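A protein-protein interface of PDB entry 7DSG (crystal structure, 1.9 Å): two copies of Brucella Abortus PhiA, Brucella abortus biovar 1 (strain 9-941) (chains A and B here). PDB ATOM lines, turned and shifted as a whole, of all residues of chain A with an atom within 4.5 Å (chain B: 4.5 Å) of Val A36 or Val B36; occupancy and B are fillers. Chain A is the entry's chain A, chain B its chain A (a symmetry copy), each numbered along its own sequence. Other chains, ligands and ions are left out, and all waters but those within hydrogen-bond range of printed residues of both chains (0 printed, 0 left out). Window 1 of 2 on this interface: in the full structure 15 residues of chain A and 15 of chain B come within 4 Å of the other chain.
The side-chain hydroxyl (OG1) of Thr A24 lies within hydrogen-bond range of the side-chain sulfur (SD) of Met B43, at 3.3 Å.
O of Pro B22 lies close to SD of Met A43, at 3.8 Å.
The backbone carbonyl oxygen of Pro A22 lies close to the side-chain sulfur of Met B43 (3.8 Å).
SD of Met A43 sits at hydrogen-bond distance from OG1 of Thr B24.
The backbone NH (N) of Ile A26 is in hydrogen-bond range of the backbone carbonyl oxygen (O) of Ala A34 (2.8 Å).
The backbone carbonyl oxygen of Val A36 is in hydrogen-bond range of the backbone NH of Thr A24 (2.7 Å).
The backbone carbonyl oxygen (O) of Val B36 lies within hydrogen-bond range of the backbone NH (N) of Thr B24 (2.7 Å).
N of Ile B26 sits at hydrogen-bond distance from O of Ala B34 (2.8 Å).
Met B43 touches Val A23.
CG2 of Thr A24 touches CG2 of Val B36, 3.6 Å away.
Ile A26 touches Ile B26.
Thr B24 touches Val A36 (CG2 to CG2, 3.6 Å).
CG1 of Val A36 touches CG1 of Val B36 (3.7 Å).
Met B43 touches Val A36 (SD to O, 3.9 Å).
CE of Met A43 touches N of Val B23, at 3.1 Å.
SD of Met A43 touches O of Val B36, at 3.9 Å.
Of the printed residues of chain B, Thr A24 touches Val B36 and Met B43.
Ala A34 touches none of the printed residues of chain B.
Ala A35 touches none of the printed residues of chain B.
Val A36 touches just these residues of chain B: Thr B24, Val B36 and Met B43.
Of the printed residues of chain A, Ile B26 touches Ile A26 (3.7 Å).
Of chain A, only Thr A24, Val A36 and Met A43 come within 4 Å of Val B36.
Of the printed residues of chain A, Met B43 touches Pro A22, Val A23, Thr A24 and Val A36.
The nearest residue of chain B that does not touch Val A36 is Ile B26 (4.4 Å).
The nearest residue of chain A that does not touch Val B36 is Ile A26 (4.4 Å).
The nearest printed residue of chain A that does not touch Thr B24 is Val A44 (5.3 Å).
Printed residues of chain A that touch a printed residue of chain B: Pro A22, Val A23, Thr A24, Ile A26, Val A36 and Met A43.
Hydrophobic or aromatic side chains of chain B within 4 Å of the printed part of chain A: Pro B22, Ile B26, Val B36 and Met B43.
Along chain B the printed residues that touch a printed residue of chain A span positions 22 to 43.
Among the printed residues, 12 pairs touch across the chains.
Among the printed residues, no Asp or Glu carboxylate lies within 4 Å of a Lys or Arg side-chain nitrogen of the other chain.
Thr A24 touches Met B43, and with the chains exchanged Met A43 touches Thr B24.
Ile A26 touches its own counterpart, Ile B26.
Val A36 touches its own counterpart, Val B36.
Val A36 touches Met B43, and with the chains exchanged Met A43 touches Val B36.
Of the 12 pairs that touch across the chains among the printed residues, 12 have their exchanged pair printed and touching as well.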
ATOM      1  N   PRO A  22     -23.701 -12.378 -18.948  1.00  0.00           N
ATOM      2  CA  PRO A  22     -22.962 -11.873 -20.103  1.00  0.00           C
ATOM      3  C   PRO A  22     -23.628 -10.601 -20.587  1.00  0.00           C
ATOM      4  O   PRO A  22     -24.857 -10.512 -20.655  1.00  0.00           O
ATOM      5  CB  PRO A  22     -23.093 -13.005 -21.126  1.00  0.00           C
ATOM      6  CG  PRO A  22     -24.373 -13.680 -20.775  1.00  0.00           C
ATOM      7  CD  PRO A  22     -24.580 -13.511 -19.297  1.00  0.00           C
ATOM      8  N   VAL A  23     -22.808  -9.604 -20.908  1.00  0.00           N
ATOM      9  CA  VAL A  23     -23.290  -8.307 -21.366  1.00  0.00           C
ATOM     10  C   VAL A  23     -22.543  -7.938 -22.642  1.00  0.00           C
ATOM     11  O   VAL A  23     -21.336  -8.183 -22.767  1.00  0.00           O
ATOM     12  CB  VAL A  23     -23.099  -7.194 -20.315  1.00  0.00           C
ATOM     13  CG1 VAL A  23     -23.651  -5.844 -20.845  1.00  0.00           C
ATOM     14  CG2 VAL A  23     -23.742  -7.551 -18.990  1.00  0.00           C
ATOM     15  N   THR A  24     -23.274  -7.413 -23.612  1.00  0.00           N
ATOM     16  CA  THR A  24     -22.678  -6.691 -24.729  1.00  0.00           C
ATOM     17  C   THR A  24     -23.033  -5.224 -24.549  1.00  0.00           C
ATOM     18  O   THR A  24     -24.215  -4.871 -24.481  1.00  0.00           O
ATOM     19  CB  THR A  24     -23.169  -7.214 -26.082  1.00  0.00           C
ATOM     20  OG1 THR A  24     -22.908  -8.628 -26.182  1.00  0.00           O
ATOM     21  CG2 THR A  24     -22.417  -6.527 -27.209  1.00  0.00           C
ATOM     22  N   ILE A  26     -22.876  -1.544 -26.310  1.00  0.00           N
ATOM     23  CA  ILE A  26     -22.765  -0.873 -27.594  1.00  0.00           C
ATOM     24  C   ILE A  26     -22.695   0.615 -27.287  1.00  0.00           C
ATOM     25  O   ILE A  26     -23.566   1.152 -26.590  1.00  0.00           O
ATOM     26  CB  ILE A  26     -23.941  -1.204 -28.531  1.00  0.00           C
ATOM     27  CG1 ILE A  26     -23.967  -2.713 -28.834  1.00  0.00           C
ATOM     28  CG2 ILE A  26     -23.806  -0.423 -29.851  1.00  0.00           C
ATOM     29  CD1 ILE A  26     -24.791  -3.529 -27.846  1.00  0.00           C
ATOM     30  N   ALA A  34     -26.452   1.246 -25.822  1.00  0.00           N
ATOM     31  CA  ALA A  34     -27.226   0.031 -25.634  1.00  0.00           C
ATOM     32  C   ALA A  34     -26.433  -0.954 -24.805  1.00  0.00           C
ATOM     33  O   ALA A  34     -25.197  -0.938 -24.791  1.00  0.00           O
ATOM     34  CB  ALA A  34     -27.602  -0.614 -26.963  1.00  0.00           C
ATOM     35  N   ALA A  35     -27.170  -1.807 -24.104  1.00  0.00           N
ATOM     36  CA  ALA A  35     -26.611  -2.997 -23.494  1.00  0.00           C
ATOM     37  C   ALA A  35     -27.547  -4.151 -23.818  1.00  0.00           C
ATOM     38  O   ALA A  35     -28.769  -3.974 -23.864  1.00  0.00           O
ATOM     39  CB  ALA A  35     -26.446  -2.836 -21.985  1.00  0.00           C
ATOM     40  N   VAL A  36     -26.969  -5.311 -24.105  1.00  0.00           N
ATOM     41  CA  VAL A  36     -27.722  -6.545 -24.266  1.00  0.00           C
ATOM     42  C   VAL A  36     -27.177  -7.518 -23.242  1.00  0.00           C
ATOM     43  O   VAL A  36     -25.962  -7.719 -23.167  1.00  0.00           O
ATOM     44  CB  VAL A  36     -27.588  -7.142 -25.679  1.00  0.00           C
ATOM     45  CG1 VAL A  36     -28.362  -8.480 -25.769  1.00  0.00           C
ATOM     46  CG2 VAL A  36     -28.027  -6.127 -26.736  1.00  0.00           C
ATOM     47  N   LEU A  37     -28.065  -8.123 -22.463  1.00  0.00           N
ATOM     48  CA  LEU A  37     -27.600  -9.098 -21.497  1.00  0.00           C
ATOM     49  C   LEU A  37     -28.500 -10.323 -21.513  1.00  0.00           C
ATOM     50  O   LEU A  37     -29.632 -10.296 -22.001  1.00  0.00           O
ATOM     51  CB  LEU A  37     -27.514  -8.499 -20.096  1.00  0.00           C
ATOM     52  CG  LEU A  37     -28.661  -7.661 -19.566  1.00  0.00           C
ATOM     53  CD1 LEU A  37     -29.622  -8.568 -18.877  1.00  0.00           C
ATOM     54  CD2 LEU A  37     -28.112  -6.611 -18.601  1.00  0.00           C
ATOM     55  N   MET A  43     -32.833 -12.982 -23.294  1.00  0.00           N
ATOM     56  CA  MET A  43     -32.025 -11.915 -23.872  1.00  0.00           C
ATOM     57  C   MET A  43     -32.749 -10.600 -23.646  1.00  0.00           C
ATOM     58  O   MET A  43     -33.885 -10.426 -24.106  1.00  0.00           O
ATOM     59  CB  MET A  43     -31.806 -12.138 -25.362  1.00  0.00           C
ATOM     60  CG  MET A  43     -31.176 -10.904 -26.056  1.00  0.00           C
ATOM     61  SD  MET A  43     -30.651 -11.272 -27.714  1.00  0.00           S
ATOM     62  CE  MET A  43     -32.130 -11.237 -28.459  1.00  0.00           C
ATOM     63  N   VAL A  44     -32.101  -9.676 -22.947  1.00  0.00           N
ATOM     64  CA  VAL A  44     -32.719  -8.420 -22.541  1.00  0.00           C
ATOM     65  C   VAL A  44     -31.964  -7.285 -23.231  1.00  0.00           C
ATOM     66  O   VAL A  44     -30.771  -7.078 -22.979  1.00  0.00           O
ATOM     67  CB  VAL A  44     -32.700  -8.257 -21.012  1.00  0.00           C
ATOM     68  CG1 VAL A  44     -33.261  -6.892 -20.613  1.00  0.00           C
ATOM     69  CG2 VAL A  44     -33.498  -9.389 -20.338  1.00  0.00           C
ATOM     70  N   PRO B  22     -32.383 -15.797 -30.554  1.00  0.00           N
ATOM     71  CA  PRO B  22     -32.760 -14.424 -30.222  1.00  0.00           C
ATOM     72  C   PRO B  22     -31.669 -13.491 -30.706  1.00  0.00           C
ATOM     73  O   PRO B  22     -30.477 -13.771 -30.554  1.00  0.00           O
ATOM     74  CB  PRO B  22     -32.851 -14.445 -28.694  1.00  0.00           C
ATOM     75  CG  PRO B  22     -31.908 -15.520 -28.277  1.00  0.00           C
ATOM     76  CD  PRO B  22     -31.864 -16.533 -29.385  1.00  0.00           C
ATOM     77  N   VAL B  23     -32.083 -12.381 -31.310  1.00  0.00           N
ATOM     78  CA  VAL B  23     -31.161 -11.391 -31.854  1.00  0.00           C
ATOM     79  C   VAL B  23     -31.572 -10.016 -31.343  1.00  0.00           C
ATOM     80  O   VAL B  23     -32.765  -9.702 -31.249  1.00  0.00           O
ATOM     81  CB  VAL B  23     -31.136 -11.384 -33.397  1.00  0.00           C
ATOM     82  CG1 VAL B  23     -30.121 -10.334 -33.920  1.00  0.00           C
ATOM     83  CG2 VAL B  23     -30.826 -12.755 -33.964  1.00  0.00           C
ATOM     84  N   THR B  24     -30.587  -9.224 -30.952  1.00  0.00           N
ATOM     85  CA  THR B  24     -30.767  -7.787 -30.781  1.00  0.00           C
ATOM     86  C   THR B  24     -29.999  -7.108 -31.903  1.00  0.00           C
ATOM     87  O   THR B  24     -28.787  -7.306 -32.039  1.00  0.00           O
ATOM     88  CB  THR B  24     -30.284  -7.304 -29.411  1.00  0.00           C
ATOM     89  OG1 THR B  24     -30.958  -8.036 -28.369  1.00  0.00           O
ATOM     90  CG2 THR B  24     -30.620  -5.834 -29.231  1.00  0.00           C
ATOM     91  N   ILE B  26     -28.750  -3.497 -33.341  1.00  0.00           N
ATOM     92  CA  ILE B  26     -28.468  -2.125 -32.953  1.00  0.00           C
ATOM     93  C   ILE B  26     -28.110  -1.390 -34.236  1.00  0.00           C
ATOM     94  O   ILE B  26     -27.219  -1.824 -34.978  1.00  0.00           O
ATOM     95  CB  ILE B  26     -27.338  -2.032 -31.912  1.00  0.00           C
ATOM     96  CG1 ILE B  26     -27.745  -2.770 -30.623  1.00  0.00           C
ATOM     97  CG2 ILE B  26     -27.038  -0.559 -31.581  1.00  0.00           C
ATOM     98  CD1 ILE B  26     -27.363  -4.245 -30.606  1.00  0.00           C
ATOM     99  N   ALA B  34     -24.583  -3.218 -35.175  1.00  0.00           N
ATOM    100  CA  ALA B  34     -24.262  -4.355 -34.332  1.00  0.00           C
ATOM    101  C   ALA B  34     -25.431  -5.316 -34.307  1.00  0.00           C
ATOM    102  O   ALA B  34     -26.589  -4.928 -34.498  1.00  0.00           O
ATOM    103  CB  ALA B  34     -23.929  -3.930 -32.907  1.00  0.00           C
ATOM    104  N   ALA B  35     -25.102  -6.582 -34.078  1.00  0.00           N
ATOM    105  CA  ALA B  35     -26.083  -7.588 -33.726  1.00  0.00           C
ATOM    106  C   ALA B  35     -25.521  -8.373 -32.551  1.00  0.00           C
ATOM    107  O   ALA B  35     -24.312  -8.612 -32.477  1.00  0.00           O
ATOM    108  CB  ALA B  35     -26.395  -8.511 -34.900  1.00  0.00           C
ATOM    109  N   VAL B  36     -26.388  -8.713 -31.606  1.00  0.00           N
ATOM    110  CA  VAL B  36     -26.045  -9.607 -30.510  1.00  0.00           C
ATOM    111  C   VAL B  36     -27.003 -10.777 -30.594  1.00  0.00           C
ATOM    112  O   VAL B  36     -28.218 -10.576 -30.669  1.00  0.00           O
ATOM    113  CB  VAL B  36     -26.164  -8.931 -29.132  1.00  0.00           C
ATOM    114  CG1 VAL B  36     -25.844  -9.948 -28.008  1.00  0.00           C
ATOM    115  CG2 VAL B  36     -25.288  -7.679 -29.070  1.00  0.00           C
ATOM    116  N   LEU B  37     -26.465 -11.990 -30.576  1.00  0.00           N
ATOM    117  CA  LEU B  37     -27.341 -13.145 -30.607  1.00  0.00           C
ATOM    118  C   LEU B  37     -26.877 -14.183 -29.598  1.00  0.00           C
ATOM    119  O   LEU B  37     -25.738 -14.173 -29.127  1.00  0.00           O
ATOM    120  CB  LEU B  37     -27.427 -13.742 -32.010  1.00  0.00           C
ATOM    121  CG  LEU B  37     -26.159 -13.955 -32.814  1.00  0.00           C
ATOM    122  CD1 LEU B  37     -25.635 -15.316 -32.507  1.00  0.00           C
ATOM    123  CD2 LEU B  37     -26.479 -13.814 -34.301  1.00  0.00           C
ATOM    124  N   MET B  43     -23.394 -15.936 -25.881  1.00  0.00           N
ATOM    125  CA  MET B  43     -23.739 -14.601 -26.357  1.00  0.00           C
ATOM    126  C   MET B  43     -22.678 -14.166 -27.351  1.00  0.00           C
ATOM    127  O   MET B  43     -21.493 -14.085 -27.003  1.00  0.00           O
ATOM    128  CB  MET B  43     -23.811 -13.610 -25.205  1.00  0.00           C
ATOM    129  CG  MET B  43     -23.920 -12.144 -25.696  1.00  0.00           C
ATOM    130  SD  MET B  43     -24.300 -11.027 -24.366  1.00  0.00           S
ATOM    131  CE  MET B  43     -22.797 -10.936 -23.676  1.00  0.00           C
ATOM    132  N   VAL B  44     -23.094 -13.882 -28.580  1.00  0.00           N
ATOM    133  CA  VAL B  44     -22.176 -13.579 -29.670  1.00  0.00           C
ATOM    134  C   VAL B  44     -22.434 -12.139 -30.110  1.00  0.00           C
ATOM    135  O   VAL B  44     -23.525 -11.816 -30.595  1.00  0.00           O
ATOM    136  CB  VAL B  44     -22.352 -14.563 -30.839  1.00  0.00           C
ATOM    137  CG1 VAL B  44     -21.452 -14.168 -32.010  1.00  0.00           C
ATOM    138  CG2 VAL B  44     -22.050 -16.003 -30.385  1.00  0.00           C
